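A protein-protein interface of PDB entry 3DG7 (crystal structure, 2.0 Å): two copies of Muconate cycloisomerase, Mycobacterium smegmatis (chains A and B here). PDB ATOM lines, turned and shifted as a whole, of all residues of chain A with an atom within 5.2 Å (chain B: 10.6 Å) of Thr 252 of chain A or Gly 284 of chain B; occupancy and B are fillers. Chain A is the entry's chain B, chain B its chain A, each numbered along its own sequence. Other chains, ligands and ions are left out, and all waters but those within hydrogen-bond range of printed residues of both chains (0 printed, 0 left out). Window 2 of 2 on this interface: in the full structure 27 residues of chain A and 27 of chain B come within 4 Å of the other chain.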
ATOM      1  N   PRO A 248      11.188 -27.990  26.976  1.00  0.00           N
ATOM      2  CA  PRO A 248      11.038 -27.753  25.538  1.00  0.00           C
ATOM      3  C   PRO A 248      11.663 -28.898  24.735  1.00  0.00           C
ATOM      4  O   PRO A 248      11.127 -29.297  23.704  1.00  0.00           O
ATOM      5  CB  PRO A 248      11.772 -26.430  25.331  1.00  0.00           C
ATOM      6  CG  PRO A 248      11.482 -25.701  26.623  1.00  0.00           C
ATOM      7  CD  PRO A 248      11.718 -26.788  27.650  1.00  0.00           C
ATOM      8  N   ALA A 249      12.796 -29.423  25.204  1.00  0.00           N
ATOM      9  CA  ALA A 249      13.457 -30.531  24.504  1.00  0.00           C
ATOM     10  C   ALA A 249      12.531 -31.751  24.430  1.00  0.00           C
ATOM     11  O   ALA A 249      12.499 -32.451  23.418  1.00  0.00           O
ATOM     12  CB  ALA A 249      14.768 -30.903  25.207  1.00  0.00           C
ATOM     13  N   ASP A 250      11.789 -32.006  25.503  1.00  0.00           N
ATOM     14  CA  ASP A 250      10.852 -33.129  25.534  1.00  0.00           C
ATOM     15  C   ASP A 250       9.722 -32.862  24.548  1.00  0.00           C
ATOM     16  O   ASP A 250       9.255 -33.773  23.872  1.00  0.00           O
ATOM     17  CB  ASP A 250      10.270 -33.330  26.936  1.00  0.00           C
ATOM     18  CG  ASP A 250      11.297 -33.846  27.928  1.00  0.00           C
ATOM     19  OD1 ASP A 250      11.936 -34.886  27.654  1.00  0.00           O
ATOM     20  OD2 ASP A 250      11.459 -33.209  28.986  1.00  0.00           O
ATOM     21  N   VAL A 251       9.273 -31.611  24.479  1.00  0.00           N
ATOM     22  CA  VAL A 251       8.217 -31.251  23.542  1.00  0.00           C
ATOM     23  C   VAL A 251       8.676 -31.609  22.125  1.00  0.00           C
ATOM     24  O   VAL A 251       7.934 -32.215  21.354  1.00  0.00           O
ATOM     25  CB  VAL A 251       7.896 -29.736  23.589  1.00  0.00           C
ATOM     26  CG1 VAL A 251       6.952 -29.367  22.444  1.00  0.00           C
ATOM     27  CG2 VAL A 251       7.246 -29.374  24.923  1.00  0.00           C
ATOM     28  N   THR A 252       9.907 -31.239  21.788  1.00  0.00           N
ATOM     29  CA  THR A 252      10.429 -31.527  20.457  1.00  0.00           C
ATOM     30  C   THR A 252      10.519 -33.028  20.191  1.00  0.00           C
ATOM     31  O   THR A 252      10.048 -33.511  19.157  1.00  0.00           O
ATOM     32  CB  THR A 252      11.816 -30.870  20.249  1.00  0.00           C
ATOM     33  OG1 THR A 252      11.672 -29.441  20.279  1.00  0.00           O
ATOM     34  CG2 THR A 252      12.417 -31.280  18.904  1.00  0.00           C
ATOM     35  N   ARG A 253      11.111 -33.769  21.124  1.00  0.00           N
ATOM     36  CA  ARG A 253      11.239 -35.215  20.954  1.00  0.00           C
ATOM     37  C   ARG A 253       9.900 -35.937  20.848  1.00  0.00           C
ATOM     38  O   ARG A 253       9.730 -36.799  19.983  1.00  0.00           O
ATOM     39  CB  ARG A 253      12.035 -35.832  22.108  1.00  0.00           C
ATOM     40  CG  ARG A 253      13.539 -35.643  22.013  1.00  0.00           C
ATOM     41  CD  ARG A 253      14.233 -36.492  23.078  1.00  0.00           C
ATOM     42  NE  ARG A 253      13.998 -35.964  24.420  1.00  0.00           N
ATOM     43  CZ  ARG A 253      14.777 -35.062  25.010  1.00  0.00           C
ATOM     44  NH1 ARG A 253      15.843 -34.596  24.378  1.00  0.00           N
ATOM     45  NH2 ARG A 253      14.483 -34.619  26.225  1.00  0.00           N
ATOM     46  N   GLU A 254       8.957 -35.601  21.727  1.00  0.00           N
ATOM     47  CA  GLU A 254       7.650 -36.262  21.722  1.00  0.00           C
ATOM     48  C   GLU A 254       6.794 -35.895  20.507  1.00  0.00           C
ATOM     49  O   GLU A 254       6.112 -36.748  19.937  1.00  0.00           O
ATOM     50  CB  GLU A 254       6.878 -35.935  23.008  1.00  0.00           C
ATOM     51  CG  GLU A 254       7.596 -36.320  24.318  1.00  0.00           C
ATOM     52  CD  GLU A 254       7.816 -37.824  24.483  1.00  0.00           C
ATOM     53  OE1 GLU A 254       6.861 -38.599  24.270  1.00  0.00           O
ATOM     54  OE2 GLU A 254       8.940 -38.232  24.848  1.00  0.00           O
ATOM     55  N   VAL A 255       6.815 -34.627  20.119  1.00  0.00           N
ATOM     56  CA  VAL A 255       6.032 -34.193  18.969  1.00  0.00           C
ATOM     57  C   VAL A 255       6.588 -34.739  17.654  1.00  0.00           C
ATOM     58  O   VAL A 255       5.838 -35.281  16.836  1.00  0.00           O
ATOM     59  CB  VAL A 255       5.954 -32.651  18.908  1.00  0.00           C
ATOM     60  CG1 VAL A 255       5.367 -32.208  17.583  1.00  0.00           C
ATOM     61  CG2 VAL A 255       5.088 -32.142  20.051  1.00  0.00           C
ATOM     62  N   LEU A 256       7.895 -34.615  17.442  1.00  0.00           N
ATOM     63  CA  LEU A 256       8.481 -35.121  16.201  1.00  0.00           C
ATOM     64  C   LEU A 256       8.423 -36.645  16.159  1.00  0.00           C
ATOM     65  O   LEU A 256       8.357 -37.242  15.082  1.00  0.00           O
ATOM     66  CB  LEU A 256       9.931 -34.654  16.052  1.00  0.00           C
ATOM     67  CG  LEU A 256      10.114 -33.136  15.944  1.00  0.00           C
ATOM     68  CD1 LEU A 256      11.586 -32.811  15.708  1.00  0.00           C
ATOM     69  CD2 LEU A 256       9.252 -32.599  14.805  1.00  0.00           C
ATOM     70  N   GLY A 257       8.433 -37.266  17.334  1.00  0.00           N
ATOM     71  CA  GLY A 257       8.374 -38.717  17.412  1.00  0.00           C
ATOM     72  C   GLY A 257       6.964 -39.265  17.249  1.00  0.00           C
ATOM     73  O   GLY A 257       6.771 -40.466  17.029  1.00  0.00           O
ATOM     74  N   LEU A 281       7.573 -22.478  21.139  1.00  0.00           N
ATOM     75  CA  LEU A 281       7.943 -23.695  20.423  1.00  0.00           C
ATOM     76  C   LEU A 281       6.666 -24.351  19.880  1.00  0.00           C
ATOM     77  O   LEU A 281       6.609 -24.740  18.712  1.00  0.00           O
ATOM     78  CB  LEU A 281       8.684 -24.659  21.361  1.00  0.00           C
ATOM     79  CG  LEU A 281       9.031 -26.050  20.811  1.00  0.00           C
ATOM     80  CD1 LEU A 281       9.877 -25.928  19.546  1.00  0.00           C
ATOM     81  CD2 LEU A 281       9.779 -26.840  21.881  1.00  0.00           C
ATOM     82  N   LEU A 285       5.722 -24.735  15.942  1.00  0.00           N
ATOM     83  CA  LEU A 285       5.532 -26.064  15.359  1.00  0.00           C
ATOM     84  C   LEU A 285       4.101 -26.239  14.861  1.00  0.00           C
ATOM     85  O   LEU A 285       3.840 -27.066  13.989  1.00  0.00           O
ATOM     86  CB  LEU A 285       5.845 -27.149  16.392  1.00  0.00           C
ATOM     87  CG  LEU A 285       7.325 -27.286  16.754  1.00  0.00           C
ATOM     88  CD1 LEU A 285       7.494 -28.339  17.841  1.00  0.00           C
ATOM     89  CD2 LEU A 285       8.113 -27.665  15.503  1.00  0.00           C
ATOM     90  N   VAL B 251      10.630 -21.174   9.407  1.00  0.00           N
ATOM     91  CA  VAL B 251      11.707 -21.863  10.112  1.00  0.00           C
ATOM     92  C   VAL B 251      11.321 -23.337  10.268  1.00  0.00           C
ATOM     93  O   VAL B 251      12.123 -24.228  10.003  1.00  0.00           O
ATOM     94  CB  VAL B 251      11.949 -21.265  11.521  1.00  0.00           C
ATOM     95  CG1 VAL B 251      12.913 -22.154  12.309  1.00  0.00           C
ATOM     96  CG2 VAL B 251      12.528 -19.858  11.407  1.00  0.00           C
ATOM     97  N   THR B 252      10.085 -23.587  10.687  1.00  0.00           N
ATOM     98  CA  THR B 252       9.628 -24.960  10.871  1.00  0.00           C
ATOM     99  C   THR B 252       9.627 -25.743   9.563  1.00  0.00           C
ATOM    100  O   THR B 252      10.155 -26.859   9.499  1.00  0.00           O
ATOM    101  CB  THR B 252       8.217 -25.000  11.504  1.00  0.00           C
ATOM    102  OG1 THR B 252       8.279 -24.460  12.834  1.00  0.00           O
ATOM    103  CG2 THR B 252       7.695 -26.435  11.577  1.00  0.00           C
ATOM    104  N   VAL B 255      13.402 -26.186   8.229  1.00  0.00           N
ATOM    105  CA  VAL B 255      14.206 -27.065   9.074  1.00  0.00           C
ATOM    106  C   VAL B 255      13.732 -28.520   9.016  1.00  0.00           C
ATOM    107  O   VAL B 255      14.541 -29.433   8.833  1.00  0.00           O
ATOM    108  CB  VAL B 255      14.207 -26.571  10.538  1.00  0.00           C
ATOM    109  CG1 VAL B 255      14.818 -27.620  11.446  1.00  0.00           C
ATOM    110  CG2 VAL B 255      15.012 -25.278  10.636  1.00  0.00           C
ATOM    111  N   LEU B 256      12.430 -28.745   9.165  1.00  0.00           N
ATOM    112  CA  LEU B 256      11.912 -30.110   9.113  1.00  0.00           C
ATOM    113  C   LEU B 256      12.058 -30.685   7.710  1.00  0.00           C
ATOM    114  O   LEU B 256      12.211 -31.898   7.541  1.00  0.00           O
ATOM    115  CB  LEU B 256      10.444 -30.152   9.544  1.00  0.00           C
ATOM    116  CG  LEU B 256      10.187 -29.725  10.993  1.00  0.00           C
ATOM    117  CD1 LEU B 256       8.708 -29.898  11.327  1.00  0.00           C
ATOM    118  CD2 LEU B 256      11.053 -30.557  11.936  1.00  0.00           C
ATOM    119  N   ILE B 263      19.756 -20.988  11.735  1.00  0.00           N
ATOM    120  CA  ILE B 263      18.825 -19.890  11.508  1.00  0.00           C
ATOM    121  C   ILE B 263      19.364 -18.484  11.752  1.00  0.00           C
ATOM    122  O   ILE B 263      19.942 -18.193  12.797  1.00  0.00           O
ATOM    123  CB  ILE B 263      17.571 -20.061  12.398  1.00  0.00           C
ATOM    124  CG1 ILE B 263      16.892 -21.406  12.103  1.00  0.00           C
ATOM    125  CG2 ILE B 263      16.603 -18.899  12.176  1.00  0.00           C
ATOM    126  CD1 ILE B 263      16.374 -21.546  10.685  1.00  0.00           C
ATOM    127  N   ILE B 265      18.729 -14.659  12.545  1.00  0.00           N
ATOM    128  CA  ILE B 265      17.708 -13.848  13.196  1.00  0.00           C
ATOM    129  C   ILE B 265      18.041 -12.393  12.877  1.00  0.00           C
ATOM    130  O   ILE B 265      19.155 -11.928  13.143  1.00  0.00           O
ATOM    131  CB  ILE B 265      17.695 -14.021  14.730  1.00  0.00           C
ATOM    132  CG1 ILE B 265      17.308 -15.462  15.103  1.00  0.00           C
ATOM    133  CG2 ILE B 265      16.685 -13.043  15.351  1.00  0.00           C
ATOM    134  CD1 ILE B 265      17.188 -15.699  16.611  1.00  0.00           C
ATOM    135  N   SER B 275      11.234 -11.841  17.038  1.00  0.00           N
ATOM    136  CA  SER B 275      12.545 -12.471  17.142  1.00  0.00           C
ATOM    137  C   SER B 275      12.617 -13.412  18.339  1.00  0.00           C
ATOM    138  O   SER B 275      13.327 -14.415  18.295  1.00  0.00           O
ATOM    139  CB  SER B 275      13.647 -11.412  17.224  1.00  0.00           C
ATOM    140  OG  SER B 275      13.789 -10.749  15.975  1.00  0.00           O
ATOM    141  N   THR B 276      11.889 -13.093  19.406  1.00  0.00           N
ATOM    142  CA  THR B 276      11.877 -13.959  20.576  1.00  0.00           C
ATOM    143  C   THR B 276      11.220 -15.281  20.173  1.00  0.00           C
ATOM    144  O   THR B 276      11.645 -16.350  20.610  1.00  0.00           O
ATOM    145  CB  THR B 276      11.091 -13.337  21.754  1.00  0.00           C
ATOM    146  OG1 THR B 276      11.702 -12.094  22.140  1.00  0.00           O
ATOM    147  CG2 THR B 276      11.096 -14.285  22.956  1.00  0.00           C
ATOM    148  N   ARG B 277      10.186 -15.208  19.333  1.00  0.00           N
ATOM    149  CA  ARG B 277       9.506 -16.420  18.876  1.00  0.00           C
ATOM    150  C   ARG B 277      10.459 -17.278  18.045  1.00  0.00           C
ATOM    151  O   ARG B 277      10.460 -18.500  18.161  1.00  0.00           O
ATOM    152  CB  ARG B 277       8.252 -16.063  18.059  1.00  0.00           C
ATOM    153  CG  ARG B 277       7.031 -15.703  18.920  1.00  0.00           C
ATOM    154  CD  ARG B 277       5.873 -15.232  18.057  1.00  0.00           C
ATOM    155  NE  ARG B 277       4.556 -15.384  18.684  1.00  0.00           N
ATOM    156  CZ  ARG B 277       4.073 -14.625  19.667  1.00  0.00           C
ATOM    157  NH1 ARG B 277       4.794 -13.634  20.182  1.00  0.00           N
ATOM    158  NH2 ARG B 277       2.840 -14.835  20.105  1.00  0.00           N
ATOM    159  N   VAL B 278      11.275 -16.637  17.213  1.00  0.00           N
ATOM    160  CA  VAL B 278      12.238 -17.367  16.392  1.00  0.00           C
ATOM    161  C   VAL B 278      13.325 -17.988  17.276  1.00  0.00           C
ATOM    162  O   VAL B 278      13.677 -19.158  17.108  1.00  0.00           O
ATOM    163  CB  VAL B 278      12.898 -16.446  15.342  1.00  0.00           C
ATOM    164  CG1 VAL B 278      14.023 -17.191  14.623  1.00  0.00           C
ATOM    165  CG2 VAL B 278      11.848 -15.977  14.333  1.00  0.00           C
ATOM    166  N   HIS B 279      13.858 -17.207  18.213  1.00  0.00           N
ATOM    167  CA  HIS B 279      14.898 -17.715  19.115  1.00  0.00           C
ATOM    168  C   HIS B 279      14.422 -18.932  19.909  1.00  0.00           C
ATOM    169  O   HIS B 279      15.128 -19.941  20.002  1.00  0.00           O
ATOM    170  CB  HIS B 279      15.352 -16.623  20.097  1.00  0.00           C
ATOM    171  CG  HIS B 279      16.127 -17.153  21.267  1.00  0.00           C
ATOM    172  ND1 HIS B 279      15.526 -17.779  22.337  1.00  0.00           N
ATOM    173  CD2 HIS B 279      17.458 -17.168  21.523  1.00  0.00           C
ATOM    174  CE1 HIS B 279      16.452 -18.156  23.203  1.00  0.00           C
ATOM    175  NE2 HIS B 279      17.633 -17.796  22.731  1.00  0.00           N
ATOM    176  N   HIS B 280      13.231 -18.839  20.489  1.00  0.00           N
ATOM    177  CA  HIS B 280      12.706 -19.949  21.275  1.00  0.00           C
ATOM    178  C   HIS B 280      12.421 -21.180  20.421  1.00  0.00           C
ATOM    179  O   HIS B 280      12.601 -22.314  20.877  1.00  0.00           O
ATOM    180  CB  HIS B 280      11.450 -19.515  22.032  1.00  0.00           C
ATOM    181  CG  HIS B 280      11.732 -18.556  23.149  1.00  0.00           C
ATOM    182  ND1 HIS B 280      10.766 -18.144  24.043  1.00  0.00           N
ATOM    183  CD2 HIS B 280      12.878 -17.937  23.521  1.00  0.00           C
ATOM    184  CE1 HIS B 280      11.306 -17.316  24.920  1.00  0.00           C
ATOM    185  NE2 HIS B 280      12.586 -17.173  24.625  1.00  0.00           N
ATOM    186  N   LEU B 281      11.977 -20.961  19.186  1.00  0.00           N
ATOM    187  CA  LEU B 281      11.700 -22.077  18.287  1.00  0.00           C
ATOM    188  C   LEU B 281      13.024 -22.751  17.909  1.00  0.00           C
ATOM    189  O   LEU B 281      13.141 -23.977  17.955  1.00  0.00           O
ATOM    190  CB  LEU B 281      10.971 -21.580  17.028  1.00  0.00           C
ATOM    191  CG  LEU B 281      10.721 -22.606  15.912  1.00  0.00           C
ATOM    192  CD1 LEU B 281       9.923 -23.794  16.451  1.00  0.00           C
ATOM    193  CD2 LEU B 281       9.969 -21.930  14.767  1.00  0.00           C
ATOM    194  N   ALA B 282      14.024 -21.950  17.547  1.00  0.00           N
ATOM    195  CA  ALA B 282      15.332 -22.489  17.175  1.00  0.00           C
ATOM    196  C   ALA B 282      16.020 -23.205  18.344  1.00  0.00           C
ATOM    197  O   ALA B 282      16.655 -24.248  18.159  1.00  0.00           O
ATOM    198  CB  ALA B 282      16.229 -21.377  16.643  1.00  0.00           C
ATOM    199  N   GLU B 283      15.894 -22.649  19.543  1.00  0.00           N
ATOM    200  CA  GLU B 283      16.506 -23.256  20.723  1.00  0.00           C
ATOM    201  C   GLU B 283      15.780 -24.564  21.039  1.00  0.00           C
ATOM    202  O   GLU B 283      16.406 -25.579  21.352  1.00  0.00           O
ATOM    203  CB  GLU B 283      16.409 -22.305  21.921  1.00  0.00           C
ATOM    204  CG  GLU B 283      17.210 -22.746  23.143  1.00  0.00           C
ATOM    205  CD  GLU B 283      16.912 -21.899  24.370  1.00  0.00           C
ATOM    206  OE1 GLU B 283      15.785 -21.988  24.891  1.00  0.00           O
ATOM    207  OE2 GLU B 283      17.801 -21.135  24.806  1.00  0.00           O
ATOM    208  N   GLY B 284      14.455 -24.526  20.953  1.00  0.00           N
ATOM    209  CA  GLY B 284      13.651 -25.706  21.228  1.00  0.00           C
ATOM    210  C   GLY B 284      13.919 -26.848  20.264  1.00  0.00           C
ATOM    211  O   GLY B 284      13.926 -28.013  20.656  1.00  0.00           O
ATOM    212  N   LEU B 285      14.130 -26.514  18.998  1.00  0.00           N
ATOM    213  CA  LEU B 285      14.414 -27.517  17.972  1.00  0.00           C
ATOM    214  C   LEU B 285      15.866 -27.969  18.041  1.00  0.00           C
ATOM    215  O   LEU B 285      16.202 -29.065  17.594  1.00  0.00           O
ATOM    216  CB  LEU B 285      14.120 -26.952  16.579  1.00  0.00           C
ATOM    217  CG  LEU B 285      12.636 -26.744  16.269  1.00  0.00           C
ATOM    218  CD1 LEU B 285      12.481 -26.113  14.890  1.00  0.00           C
ATOM    219  CD2 LEU B 285      11.916 -28.091  16.335  1.00  0.00           C
ATOM    220  N   GLY B 286      16.722 -27.115  18.598  1.00  0.00           N
ATOM    221  CA  GLY B 286      18.128 -27.445  18.727  1.00  0.00           C
ATOM    222  C   GLY B 286      18.947 -27.034  17.519  1.00  0.00           C
ATOM    223  O   GLY B 286      19.692 -27.841  16.969  1.00  0.00           O
ATOM    224  N   LEU B 287      18.816 -25.773  17.116  1.00  0.00           N
ATOM    225  CA  LEU B 287      19.536 -25.249  15.959  1.00  0.00           C
ATOM    226  C   LEU B 287      20.336 -24.001  16.297  1.00  0.00           C
ATOM    227  O   LEU B 287      19.884 -23.172  17.083  1.00  0.00           O
ATOM    228  CB  LEU B 287      18.542 -24.881  14.860  1.00  0.00           C
ATOM    229  CG  LEU B 287      17.588 -25.993  14.429  1.00  0.00           C
ATOM    230  CD1 LEU B 287      16.445 -25.402  13.620  1.00  0.00           C
ATOM    231  CD2 LEU B 287      18.358 -27.029  13.631  1.00  0.00           C
ATOM    232  N   ASP B 288      21.509 -23.859  15.689  1.00  0.00           N
ATOM    233  CA  ASP B 288      22.325 -22.672  15.911  1.00  0.00           C
ATOM    234  C   ASP B 288      21.619 -21.479  15.292  1.00  0.00           C
ATOM    235  O   ASP B 288      20.881 -21.621  14.309  1.00  0.00           O
ATOM    236  CB  ASP B 288      23.699 -22.800  15.256  1.00  0.00           C
ATOM    237  CG  ASP B 288      24.628 -23.700  16.026  1.00  0.00           C
ATOM    238  OD1 ASP B 288      24.351 -23.964  17.215  1.00  0.00           O
ATOM    239  OD2 ASP B 288      25.642 -24.130  15.437  1.00  0.00           O
ATOM    240  N   MET B 289      21.855 -20.305  15.866  1.00  0.00           N
ATOM    241  CA  MET B 289      21.250 -19.076  15.374  1.00  0.00           C
ATOM    242  C   MET B 289      22.266 -17.938  15.439  1.00  0.00           C
ATOM    243  O   MET B 289      23.075 -17.869  16.365  1.00  0.00           O
ATOM    244  CB  MET B 289      19.996 -18.749  16.194  1.00  0.00           C
ATOM    245  CG  MET B 289      20.228 -18.602  17.685  1.00  0.00           C
ATOM    246  SD  MET B 289      18.688 -18.580  18.627  1.00  0.00           S
ATOM    247  CE  MET B 289      18.596 -20.323  19.144  1.00  0.00           C
ATOM    248  N   ARG B 313      22.221 -17.933  23.435  1.00  0.00           N
ATOM    249  CA  ARG B 313      22.315 -18.564  22.113  1.00  0.00           C
ATOM    250  C   ARG B 313      22.656 -17.612  20.981  1.00  0.00           C
ATOM    251  O   ARG B 313      23.267 -18.010  19.987  1.00  0.00           O
ATOM    252  CB  ARG B 313      21.017 -19.316  21.791  1.00  0.00           C
ATOM    253  CG  ARG B 313      20.737 -20.500  22.730  1.00  0.00           C
ATOM    254  CD  ARG B 313      21.610 -21.706  22.399  1.00  0.00           C
ATOM    255  NE  ARG B 313      21.383 -22.813  23.330  1.00  0.00           N
ATOM    256  CZ  ARG B 313      21.805 -24.059  23.134  1.00  0.00           C
ATOM    257  NH1 ARG B 313      22.475 -24.372  22.036  1.00  0.00           N
ATOM    258  NH2 ARG B 313      21.556 -24.997  24.041  1.00  0.00           N
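OG1 of Thr 252 of chain A is in hydrogen-bond range of O of Gly 284 of chain B, at 2.7 Å.
O of Pro 248 of chain A lies within hydrogen-bond range of OG1 of Thr 252 of chain A, 3.5 Å away.
Among the printed residues, merely in contact across the chains: Leu 281 of chain A with Leu 281 of chain B (3.8 Å), Leu 285 of chain A with Leu 285 of chain B (3.9 Å) and Leu 256 of chain A with Leu 256 of chain B (3.96 Å).
Of chain B, only Gly 284 comes within 4 Å of Thr 252 of chain A. Gly 284 of chain B touches just one residue of chain A: Thr 252 (2.7 Å). Ala 249 of chain A touches none of the printed residues of chain B. Val 255 of chain A touches none of the printed residues of chain B. Leu 256 of chain A touches just one residue of chain B: Leu 256 (3.96 Å). Printed residues of chain A within 4 Å of Leu 256 of chain B: Leu 256 (3.96 Å). Of the printed residues of chain B, Leu 281 of chain A touches Leu 281 (3.8 Å). The nearest residue of chain B that does not touch Thr 252 of chain A is Leu 285 of chain B (4.03 Å). The nearest printed residue of chain A that does not touch Leu 256 of chain B is Leu 285 of chain A (4.8 Å).
Hydrophobic or aromatic side chains of chain A within 4 Å of the printed part of chain B: Leu 256, Leu 281 and Leu 285.
Leu 256 of chain B touches its own counterpart, Leu 256 of chain A. Leu 281 of chain B touches its own counterpart, Leu 281 of chain A. Leu 285 of chain B touches its own counterpart, Leu 285 of chain A. Positions printed for both chains: 251, 252, 255, 256, 281 and 285.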
